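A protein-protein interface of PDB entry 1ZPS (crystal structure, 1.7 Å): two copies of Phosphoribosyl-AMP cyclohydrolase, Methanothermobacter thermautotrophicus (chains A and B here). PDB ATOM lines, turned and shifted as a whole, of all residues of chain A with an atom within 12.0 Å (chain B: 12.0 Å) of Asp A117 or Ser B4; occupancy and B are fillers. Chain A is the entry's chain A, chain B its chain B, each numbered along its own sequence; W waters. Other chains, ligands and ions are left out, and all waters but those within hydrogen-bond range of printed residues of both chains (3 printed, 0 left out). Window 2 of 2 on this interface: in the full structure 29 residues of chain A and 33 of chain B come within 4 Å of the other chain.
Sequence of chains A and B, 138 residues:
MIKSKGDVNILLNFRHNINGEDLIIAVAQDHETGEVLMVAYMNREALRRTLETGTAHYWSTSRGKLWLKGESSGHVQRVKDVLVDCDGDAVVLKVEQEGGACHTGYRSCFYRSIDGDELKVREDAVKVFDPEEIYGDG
CB of Ser A113 touches OD1 of Asp B81, 3.3 Å away.
Val B82 touches Ser A113 (O to CA, 3.1 Å).
Ile A114 touches Leu B51 (CD1 to CD2, 3.9 Å).
Ile A114 touches Val B84 (CG1 to CG2, 3.9 Å).
Lys B5 touches Gly A116 (CA to O, 3.6 Å).
Gly A116 touches Val B8.
CA of Asp A117 touches CG2 of Val B8, 3.4 Å away.
CD2 of Leu A119 touches CG2 of Val B84, 3.97 Å away.
N of Ser A113 is in hydrogen-bond range of O of Lys A120 (3.0 Å).
N of Ser B4 sits at hydrogen-bond distance from OD2 of Asp B7 (2.6 Å).
No position is printed for both chains.
Of the 11 pairs that touch across the chains among the printed residues, none has its exchanged pair printed and touching as well.
Water W1 lies within hydrogen-bond range of O of Ile A114 (2.7 Å), OD1 of Asp B81 (2.8 Å) and N of Val B82 (2.9 Å).
Water W3 lies within hydrogen-bond range of the backbone carbonyl oxygen (O) of Gly A116 and the backbone carbonyl oxygen (O) of Lys B5.
Water W2 lies within hydrogen-bond range of the backbone carbonyl oxygen of Val B84 (2.8 Å) and the guanidinium group of Arg A112 (2.8 Å).
Of the 10 printed residues of chain A, 6 touch a printed residue of chain B.
Hydrophobic or aromatic side chains of chain A that line the printed part of chain B: Ile A114 and Leu A119.
Among the printed residues, 11 pairs touch across the chains.
Among the printed residues, no Asp or Glu carboxylate lies within 4 Å of a Lys or Arg side-chain nitrogen of the other chain.
Printed residues of chain B within 4 Å of Arg A112: Val B84 (2.8 Å).
Printed residues of chain B within 4 Å of Ser A113: Asp B81 and Val B82.
Printed residues of chain B within 4 Å of Ile A114: Leu B51, Val B82 and Val B84.
No residue of chain B comes within 4 Å of Asp A115.
Of chain B, only Lys B5 and Val B8 come within 4 Å of Gly A116.
Asp A117 touches two residues of chain B.
No residue of chain B comes within 4 Å of Glu A118.
Leu A119 touches just one residue of chain B: Val B84.
Val A121 touches none of the printed residues of chain B.
Of the printed residues of chain A, Ser B4 touches Asp A117.
Lys B5 touches one residue of chain A.
No residue of chain A comes within 4 Å of Gly B6.
No residue of chain A comes within 4 Å of Asp B7.
Val B8 touches just these residues of chain A: Gly A116 and Asp A117.
Of the printed residues of chain A, Val B82 touches Ser A113 and Ile A114.
The nearest residue of chain B that does not touch Asp A117 is Leu B11 (4.4 Å).
The nearest residue of chain A that does not touch Ser B4 is Gly A116 (5.0 Å).
The nearest printed residue of chain A that does not touch Leu B51 is Gly A116 (6.6 Å).
N of Val B84 sits at hydrogen-bond distance from O of Arg A112 (2.8 Å).
The backbone NH (N) of Ile A114 lies within hydrogen-bond range of the backbone carbonyl oxygen (O) of Val B82, 2.9 Å away.
The backbone carbonyl oxygen (O) of Ser B4 sits close to the side-chain carboxylate (OD2) of Asp A117, 3.4 Å away.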
ATOM      1  N   ARG A 112      13.816  -0.859  29.114  1.00  0.00           N
ATOM      2  CA  ARG A 112      12.905  -1.995  29.242  1.00  0.00           C
ATOM      3  C   ARG A 112      13.686  -3.300  29.331  1.00  0.00           C
ATOM      4  O   ARG A 112      14.819  -3.393  28.858  1.00  0.00           O
ATOM      5  CB  ARG A 112      11.968  -2.089  28.032  1.00  0.00           C
ATOM      6  CG  ARG A 112      11.022  -0.921  27.860  1.00  0.00           C
ATOM      7  CD  ARG A 112      10.224  -1.078  26.574  1.00  0.00           C
ATOM      8  NE  ARG A 112      11.092  -1.011  25.402  1.00  0.00           N
ATOM      9  CZ  ARG A 112      10.697  -1.262  24.159  1.00  0.00           C
ATOM     10  NH1 ARG A 112       9.438  -1.604  23.916  1.00  0.00           N
ATOM     11  NH2 ARG A 112      11.563  -1.173  23.159  1.00  0.00           N
ATOM     12  N   SER A 113      13.071  -4.305  29.940  1.00  0.00           N
ATOM     13  CA  SER A 113      13.688  -5.614  30.054  1.00  0.00           C
ATOM     14  C   SER A 113      12.647  -6.679  29.733  1.00  0.00           C
ATOM     15  O   SER A 113      11.438  -6.429  29.800  1.00  0.00           O
ATOM     16  CB  SER A 113      14.255  -5.829  31.463  1.00  0.00           C
ATOM     17  OG  SER A 113      13.239  -5.744  32.446  1.00  0.00           O
ATOM     18  N   ILE A 114      13.112  -7.860  29.349  1.00  0.00           N
ATOM     19  CA  ILE A 114      12.199  -8.951  29.055  1.00  0.00           C
ATOM     20  C   ILE A 114      11.735  -9.479  30.402  1.00  0.00           C
ATOM     21  O   ILE A 114      12.536  -9.996  31.179  1.00  0.00           O
ATOM     22  CB  ILE A 114      12.894 -10.088  28.293  1.00  0.00           C
ATOM     23  CG1 ILE A 114      13.317  -9.600  26.909  1.00  0.00           C
ATOM     24  CG2 ILE A 114      11.960 -11.282  28.180  1.00  0.00           C
ATOM     25  CD1 ILE A 114      14.079 -10.635  26.100  1.00  0.00           C
ATOM     26  N   ASP A 115      10.446  -9.326  30.685  1.00  0.00           N
ATOM     27  CA  ASP A 115       9.899  -9.801  31.947  1.00  0.00           C
ATOM     28  C   ASP A 115       8.956 -10.961  31.677  1.00  0.00           C
ATOM     29  O   ASP A 115       7.739 -10.789  31.625  1.00  0.00           O
ATOM     30  CB  ASP A 115       9.151  -8.676  32.668  1.00  0.00           C
ATOM     31  CG  ASP A 115       8.669  -9.089  34.051  1.00  0.00           C
ATOM     32  OD1 ASP A 115       7.889 -10.059  34.149  1.00  0.00           O
ATOM     33  OD2 ASP A 115       9.072  -8.441  35.041  1.00  0.00           O
ATOM     34  N   GLY A 116       9.534 -12.143  31.492  1.00  0.00           N
ATOM     35  CA  GLY A 116       8.734 -13.321  31.236  1.00  0.00           C
ATOM     36  C   GLY A 116       8.375 -13.516  29.777  1.00  0.00           C
ATOM     37  O   GLY A 116       8.966 -14.356  29.097  1.00  0.00           O
ATOM     38  N   ASP A 117       7.415 -12.738  29.286  1.00  0.00           N
ATOM     39  CA  ASP A 117       6.983 -12.874  27.900  1.00  0.00           C
ATOM     40  C   ASP A 117       6.713 -11.533  27.213  1.00  0.00           C
ATOM     41  O   ASP A 117       6.281 -11.497  26.064  1.00  0.00           O
ATOM     42  CB  ASP A 117       5.733 -13.761  27.852  1.00  0.00           C
ATOM     43  CG  ASP A 117       5.393 -14.226  26.448  1.00  0.00           C
ATOM     44  OD1 ASP A 117       4.953 -13.394  25.629  1.00  0.00           O
ATOM     45  OD2 ASP A 117       5.568 -15.431  26.163  1.00  0.00           O
ATOM     46  N   GLU A 118       6.978 -10.430  27.907  1.00  0.00           N
ATOM     47  CA  GLU A 118       6.754  -9.109  27.326  1.00  0.00           C
ATOM     48  C   GLU A 118       7.914  -8.149  27.581  1.00  0.00           C
ATOM     49  O   GLU A 118       8.843  -8.463  28.325  1.00  0.00           O
ATOM     50  CB  GLU A 118       5.468  -8.497  27.885  1.00  0.00           C
ATOM     51  CG  GLU A 118       4.194  -9.200  27.452  1.00  0.00           C
ATOM     52  CD  GLU A 118       2.953  -8.562  28.049  1.00  0.00           C
ATOM     53  OE1 GLU A 118       2.830  -7.322  27.976  1.00  0.00           O
ATOM     54  OE2 GLU A 118       2.099  -9.300  28.585  1.00  0.00           O
ATOM     55  N   LEU A 119       7.856  -6.984  26.943  1.00  0.00           N
ATOM     56  CA  LEU A 119       8.880  -5.958  27.110  1.00  0.00           C
ATOM     57  C   LEU A 119       8.298  -4.899  28.035  1.00  0.00           C
ATOM     58  O   LEU A 119       7.470  -4.090  27.617  1.00  0.00           O
ATOM     59  CB  LEU A 119       9.236  -5.322  25.765  1.00  0.00           C
ATOM     60  CG  LEU A 119       9.705  -6.261  24.652  1.00  0.00           C
ATOM     61  CD1 LEU A 119      10.104  -5.438  23.437  1.00  0.00           C
ATOM     62  CD2 LEU A 119      10.877  -7.101  25.138  1.00  0.00           C
ATOM     63  N   LYS A 120       8.730  -4.900  29.290  1.00  0.00           N
ATOM     64  CA  LYS A 120       8.199  -3.942  30.249  1.00  0.00           C
ATOM     65  C   LYS A 120       9.218  -2.938  30.760  1.00  0.00           C
ATOM     66  O   LYS A 120      10.398  -3.250  30.918  1.00  0.00           O
ATOM     67  CB  LYS A 120       7.567  -4.697  31.422  1.00  0.00           C
ATOM     68  CG  LYS A 120       6.450  -5.636  30.987  1.00  0.00           C
ATOM     69  CD  LYS A 120       5.872  -6.420  32.153  1.00  0.00           C
ATOM     70  CE  LYS A 120       4.791  -7.379  31.675  1.00  0.00           C
ATOM     71  NZ  LYS A 120       4.208  -8.176  32.793  1.00  0.00           N
ATOM     72  N   VAL A 121       8.752  -1.720  31.009  1.00  0.00           N
ATOM     73  CA  VAL A 121       9.613  -0.667  31.514  1.00  0.00           C
ATOM     74  C   VAL A 121      10.219  -1.133  32.835  1.00  0.00           C
ATOM     75  O   VAL A 121       9.522  -1.696  33.678  1.00  0.00           O
ATOM     76  CB  VAL A 121       8.816   0.638  31.741  1.00  0.00           C
ATOM     77  CG1 VAL A 121       9.729   1.721  32.294  1.00  0.00           C
ATOM     78  CG2 VAL A 121       8.192   1.094  30.430  1.00  0.00           C
ATOM     79  N   SER B   4       6.390 -19.689  25.128  1.00  0.00           N
ATOM     80  CA  SER B   4       7.594 -19.809  26.000  1.00  0.00           C
ATOM     81  C   SER B   4       8.353 -18.491  26.087  1.00  0.00           C
ATOM     82  O   SER B   4       8.105 -17.566  25.315  1.00  0.00           O
ATOM     83  CB  SER B   4       8.531 -20.897  25.466  1.00  0.00           C
ATOM     84  OG  SER B   4       7.922 -22.173  25.523  1.00  0.00           O
ATOM     85  N   LYS B   5       9.280 -18.420  27.034  1.00  0.00           N
ATOM     86  CA  LYS B   5      10.091 -17.225  27.238  1.00  0.00           C
ATOM     87  C   LYS B   5      10.884 -16.891  25.976  1.00  0.00           C
ATOM     88  O   LYS B   5      10.963 -15.730  25.568  1.00  0.00           O
ATOM     89  CB  LYS B   5      11.059 -17.447  28.404  1.00  0.00           C
ATOM     90  CG  LYS B   5      10.385 -17.843  29.709  1.00  0.00           C
ATOM     91  CD  LYS B   5      11.407 -18.079  30.814  1.00  0.00           C
ATOM     92  CE  LYS B   5      10.727 -18.472  32.116  1.00  0.00           C
ATOM     93  NZ  LYS B   5      11.706 -18.697  33.218  1.00  0.00           N
ATOM     94  N   GLY B   6      11.465 -17.917  25.364  1.00  0.00           N
ATOM     95  CA  GLY B   6      12.257 -17.720  24.163  1.00  0.00           C
ATOM     96  C   GLY B   6      11.496 -17.136  22.987  1.00  0.00           C
ATOM     97  O   GLY B   6      12.090 -16.515  22.102  1.00  0.00           O
ATOM     98  N   ASP B   7      10.180 -17.325  22.974  1.00  0.00           N
ATOM     99  CA  ASP B   7       9.348 -16.822  21.887  1.00  0.00           C
ATOM    100  C   ASP B   7       9.243 -15.301  21.830  1.00  0.00           C
ATOM    101  O   ASP B   7       8.789 -14.742  20.830  1.00  0.00           O
ATOM    102  CB  ASP B   7       7.954 -17.442  21.973  1.00  0.00           C
ATOM    103  CG  ASP B   7       7.984 -18.948  21.824  1.00  0.00           C
ATOM    104  OD1 ASP B   7       8.539 -19.430  20.816  1.00  0.00           O
ATOM    105  OD2 ASP B   7       7.458 -19.648  22.711  1.00  0.00           O
ATOM    106  N   VAL B   8       9.666 -14.628  22.894  1.00  0.00           N
ATOM    107  CA  VAL B   8       9.620 -13.169  22.920  1.00  0.00           C
ATOM    108  C   VAL B   8      10.509 -12.614  21.807  1.00  0.00           C
ATOM    109  O   VAL B   8      10.398 -11.448  21.431  1.00  0.00           O
ATOM    110  CB  VAL B   8      10.107 -12.608  24.278  1.00  0.00           C
ATOM    111  CG1 VAL B   8      10.127 -11.088  24.244  1.00  0.00           C
ATOM    112  CG2 VAL B   8       9.196 -13.087  25.394  1.00  0.00           C
ATOM    113  N   ASN B   9      11.386 -13.461  21.275  1.00  0.00           N
ATOM    114  CA  ASN B   9      12.288 -13.045  20.208  1.00  0.00           C
ATOM    115  C   ASN B   9      11.538 -12.419  19.040  1.00  0.00           C
ATOM    116  O   ASN B   9      12.097 -11.617  18.298  1.00  0.00           O
ATOM    117  CB  ASN B   9      13.099 -14.235  19.688  1.00  0.00           C
ATOM    118  CG  ASN B   9      12.255 -15.210  18.886  1.00  0.00           C
ATOM    119  OD1 ASN B   9      11.597 -16.091  19.443  1.00  0.00           O
ATOM    120  ND2 ASN B   9      12.262 -15.047  17.570  1.00  0.00           N
ATOM    121  N   ILE B  10      10.271 -12.784  18.874  1.00  0.00           N
ATOM    122  CA  ILE B  10       9.479 -12.246  17.775  1.00  0.00           C
ATOM    123  C   ILE B  10       9.262 -10.741  17.914  1.00  0.00           C
ATOM    124  O   ILE B  10       9.002 -10.048  16.930  1.00  0.00           O
ATOM    125  CB  ILE B  10       8.100 -12.942  17.684  1.00  0.00           C
ATOM    126  CG1 ILE B  10       7.388 -12.518  16.398  1.00  0.00           C
ATOM    127  CG2 ILE B  10       7.250 -12.576  18.892  1.00  0.00           C
ATOM    128  CD1 ILE B  10       6.087 -13.246  16.149  1.00  0.00           C
ATOM    129  N   LEU B  11       9.375 -10.236  19.136  1.00  0.00           N
ATOM    130  CA  LEU B  11       9.182  -8.815  19.387  1.00  0.00           C
ATOM    131  C   LEU B  11      10.419  -7.989  19.061  1.00  0.00           C
ATOM    132  O   LEU B  11      10.330  -6.769  18.918  1.00  0.00           O
ATOM    133  CB  LEU B  11       8.775  -8.588  20.843  1.00  0.00           C
ATOM    134  CG  LEU B  11       7.440  -9.207  21.264  1.00  0.00           C
ATOM    135  CD1 LEU B  11       7.148  -8.840  22.703  1.00  0.00           C
ATOM    136  CD2 LEU B  11       6.323  -8.711  20.352  1.00  0.00           C
ATOM    137  N   LEU B  12      11.574  -8.641  18.952  1.00  0.00           N
ATOM    138  CA  LEU B  12      12.801  -7.918  18.629  1.00  0.00           C
ATOM    139  C   LEU B  12      13.046  -7.861  17.127  1.00  0.00           C
ATOM    140  O   LEU B  12      12.515  -8.675  16.363  1.00  0.00           O
ATOM    141  CB  LEU B  12      14.009  -8.531  19.345  1.00  0.00           C
ATOM    142  CG  LEU B  12      14.141  -8.144  20.825  1.00  0.00           C
ATOM    143  CD1 LEU B  12      13.076  -8.850  21.643  1.00  0.00           C
ATOM    144  CD2 LEU B  12      15.528  -8.511  21.333  1.00  0.00           C
ATOM    145  N   ARG B  44      18.422 -14.919  15.638  1.00  0.00           N
ATOM    146  CA  ARG B  44      17.203 -15.291  16.342  1.00  0.00           C
ATOM    147  C   ARG B  44      17.370 -16.500  17.259  1.00  0.00           C
ATOM    148  O   ARG B  44      16.959 -16.470  18.422  1.00  0.00           O
ATOM    149  CB  ARG B  44      16.083 -15.558  15.336  1.00  0.00           C
ATOM    150  CG  ARG B  44      14.707 -15.742  15.964  1.00  0.00           C
ATOM    151  CD  ARG B  44      13.654 -15.909  14.882  1.00  0.00           C
ATOM    152  NE  ARG B  44      13.680 -14.793  13.940  1.00  0.00           N
ATOM    153  CZ  ARG B  44      13.240 -13.569  14.215  1.00  0.00           C
ATOM    154  NH1 ARG B  44      12.728 -13.293  15.410  1.00  0.00           N
ATOM    155  NH2 ARG B  44      13.317 -12.615  13.297  1.00  0.00           N
ATOM    156  N   GLU B  45      17.975 -17.565  16.740  1.00  0.00           N
ATOM    157  CA  GLU B  45      18.160 -18.779  17.524  1.00  0.00           C
ATOM    158  C   GLU B  45      19.015 -18.572  18.777  1.00  0.00           C
ATOM    159  O   GLU B  45      18.721 -19.134  19.836  1.00  0.00           O
ATOM    160  CB  GLU B  45      18.765 -19.881  16.648  1.00  0.00           C
ATOM    161  CG  GLU B  45      18.827 -21.239  17.316  1.00  0.00           C
ATOM    162  CD  GLU B  45      17.459 -21.832  17.613  1.00  0.00           C
ATOM    163  OE1 GLU B  45      16.424 -21.187  17.328  1.00  0.00           O
ATOM    164  OE2 GLU B  45      17.419 -22.955  18.143  1.00  0.00           O
ATOM    165  N   LEU B  47      19.325 -15.862  20.557  1.00  0.00           N
ATOM    166  CA  LEU B  47      18.549 -15.168  21.575  1.00  0.00           C
ATOM    167  C   LEU B  47      17.554 -16.139  22.199  1.00  0.00           C
ATOM    168  O   LEU B  47      17.427 -16.207  23.420  1.00  0.00           O
ATOM    169  CB  LEU B  47      17.804 -13.971  20.975  1.00  0.00           C
ATOM    170  CG  LEU B  47      16.871 -13.258  21.961  1.00  0.00           C
ATOM    171  CD1 LEU B  47      17.673 -12.772  23.169  1.00  0.00           C
ATOM    172  CD2 LEU B  47      16.182 -12.094  21.274  1.00  0.00           C
ATOM    173  N   ARG B  48      16.864 -16.906  21.360  1.00  0.00           N
ATOM    174  CA  ARG B  48      15.882 -17.862  21.859  1.00  0.00           C
ATOM    175  C   ARG B  48      16.501 -18.851  22.841  1.00  0.00           C
ATOM    176  O   ARG B  48      15.927 -19.134  23.891  1.00  0.00           O
ATOM    177  CB  ARG B  48      15.249 -18.632  20.701  1.00  0.00           C
ATOM    178  CG  ARG B  48      14.039 -19.454  21.115  1.00  0.00           C
ATOM    179  CD  ARG B  48      13.587 -20.371  19.992  1.00  0.00           C
ATOM    180  NE  ARG B  48      14.557 -21.436  19.754  1.00  0.00           N
ATOM    181  CZ  ARG B  48      14.789 -22.442  20.590  1.00  0.00           C
ATOM    182  NH1 ARG B  48      14.115 -22.536  21.732  1.00  0.00           N
ATOM    183  NH2 ARG B  48      15.702 -23.356  20.287  1.00  0.00           N
ATOM    184  N   ARG B  49      17.672 -19.380  22.504  1.00  0.00           N
ATOM    185  CA  ARG B  49      18.316 -20.345  23.385  1.00  0.00           C
ATOM    186  C   ARG B  49      18.808 -19.681  24.659  1.00  0.00           C
ATOM    187  O   ARG B  49      18.810 -20.296  25.725  1.00  0.00           O
ATOM    188  CB  ARG B  49      19.467 -21.048  22.662  1.00  0.00           C
ATOM    189  CG  ARG B  49      18.998 -21.837  21.449  1.00  0.00           C
ATOM    190  CD  ARG B  49      20.091 -22.742  20.894  1.00  0.00           C
ATOM    191  NE  ARG B  49      19.663 -23.352  19.636  1.00  0.00           N
ATOM    192  CZ  ARG B  49      20.399 -24.197  18.922  1.00  0.00           C
ATOM    193  NH1 ARG B  49      21.607 -24.544  19.338  1.00  0.00           N
ATOM    194  NH2 ARG B  49      19.925 -24.689  17.783  1.00  0.00           N
ATOM    195  N   THR B  50      19.210 -18.421  24.551  1.00  0.00           N
ATOM    196  CA  THR B  50      19.684 -17.693  25.718  1.00  0.00           C
ATOM    197  C   THR B  50      18.534 -17.548  26.706  1.00  0.00           C
ATOM    198  O   THR B  50      18.703 -17.756  27.911  1.00  0.00           O
ATOM    199  CB  THR B  50      20.197 -16.300  25.330  1.00  0.00           C
ATOM    200  OG1 THR B  50      21.389 -16.440  24.548  1.00  0.00           O
ATOM    201  CG2 THR B  50      20.497 -15.467  26.586  1.00  0.00           C
ATOM    202  N   LEU B  51      17.360 -17.202  26.186  1.00  0.00           N
ATOM    203  CA  LEU B  51      16.182 -17.035  27.028  1.00  0.00           C
ATOM    204  C   LEU B  51      15.697 -18.374  27.581  1.00  0.00           C
ATOM    205  O   LEU B  51      15.196 -18.447  28.704  1.00  0.00           O
ATOM    206  CB  LEU B  51      15.061 -16.359  26.234  1.00  0.00           C
ATOM    207  CG  LEU B  51      15.365 -14.944  25.737  1.00  0.00           C
ATOM    208  CD1 LEU B  51      14.171 -14.406  24.963  1.00  0.00           C
ATOM    209  CD2 LEU B  51      15.680 -14.040  26.925  1.00  0.00           C
ATOM    210  N   GLU B  52      15.849 -19.436  26.795  1.00  0.00           N
ATOM    211  CA  GLU B  52      15.420 -20.757  27.230  1.00  0.00           C
ATOM    212  C   GLU B  52      16.278 -21.332  28.356  1.00  0.00           C
ATOM    213  O   GLU B  52      15.750 -21.846  29.342  1.00  0.00           O
ATOM    214  CB  GLU B  52      15.419 -21.734  26.045  1.00  0.00           C
ATOM    215  CG  GLU B  52      15.152 -23.193  26.440  1.00  0.00           C
ATOM    216  CD  GLU B  52      15.150 -24.139  25.247  1.00  0.00           C
ATOM    217  OE1 GLU B  52      14.314 -23.955  24.344  1.00  0.00           O
ATOM    218  OE2 GLU B  52      15.986 -25.065  25.215  1.00  0.00           O
ATOM    219  N   THR B  53      17.596 -21.236  28.214  1.00  0.00           N
ATOM    220  CA  THR B  53      18.515 -21.791  29.207  1.00  0.00           C
ATOM    221  C   THR B  53      18.994 -20.827  30.285  1.00  0.00           C
ATOM    222  O   THR B  53      19.423 -21.254  31.356  1.00  0.00           O
ATOM    223  CB  THR B  53      19.767 -22.370  28.527  1.00  0.00           C
ATOM    224  OG1 THR B  53      20.501 -21.312  27.898  1.00  0.00           O
ATOM    225  CG2 THR B  53      19.375 -23.398  27.473  1.00  0.00           C
ATOM    226  N   GLY B  54      18.928 -19.531  30.010  1.00  0.00           N
ATOM    227  CA  GLY B  54      19.400 -18.571  30.990  1.00  0.00           C
ATOM    228  C   GLY B  54      20.918 -18.483  30.946  1.00  0.00           C
ATOM    229  O   GLY B  54      21.557 -18.043  31.903  1.00  0.00           O
ATOM    230  N   ASP B  81      19.301 -10.836  33.671  1.00  0.00           N
ATOM    231  CA  ASP B  81      18.341  -9.867  33.155  1.00  0.00           C
ATOM    232  C   ASP B  81      18.694  -9.583  31.699  1.00  0.00           C
ATOM    233  O   ASP B  81      19.859  -9.647  31.327  1.00  0.00           O
ATOM    234  CB  ASP B  81      18.451  -8.566  33.954  1.00  0.00           C
ATOM    235  CG  ASP B  81      17.187  -7.727  33.911  1.00  0.00           C
ATOM    236  OD1 ASP B  81      16.490  -7.725  32.873  1.00  0.00           O
ATOM    237  OD2 ASP B  81      16.901  -7.049  34.922  1.00  0.00           O
ATOM    238  N   VAL B  82      17.691  -9.278  30.884  1.00  0.00           N
ATOM    239  CA  VAL B  82      17.921  -8.948  29.480  1.00  0.00           C
ATOM    240  C   VAL B  82      17.237  -7.618  29.190  1.00  0.00           C
ATOM    241  O   VAL B  82      16.007  -7.541  29.163  1.00  0.00           O
ATOM    242  CB  VAL B  82      17.338 -10.018  28.525  1.00  0.00           C
ATOM    243  CG1 VAL B  82      17.565  -9.601  27.074  1.00  0.00           C
ATOM    244  CG2 VAL B  82      17.996 -11.365  28.785  1.00  0.00           C
ATOM    245  N   VAL B  84      16.373  -4.385  26.739  1.00  0.00           N
ATOM    246  CA  VAL B  84      16.158  -4.211  25.306  1.00  0.00           C
ATOM    247  C   VAL B  84      16.212  -2.751  24.852  1.00  0.00           C
ATOM    248  O   VAL B  84      15.723  -1.853  25.544  1.00  0.00           O
ATOM    249  CB  VAL B  84      14.809  -4.830  24.905  1.00  0.00           C
ATOM    250  CG1 VAL B  84      14.615  -4.751  23.409  1.00  0.00           C
ATOM    251  CG2 VAL B  84      14.752  -6.284  25.382  1.00  0.00           C
HETATM  252  O   HOH W   1      15.105 -10.000  31.936  1.00  0.00           O
HETATM  253  O   HOH W   2      13.708   0.081  25.558  1.00  0.00           O
HETATM  254  O   HOH W   3      11.547 -14.643  28.106  1.00  0.00           O
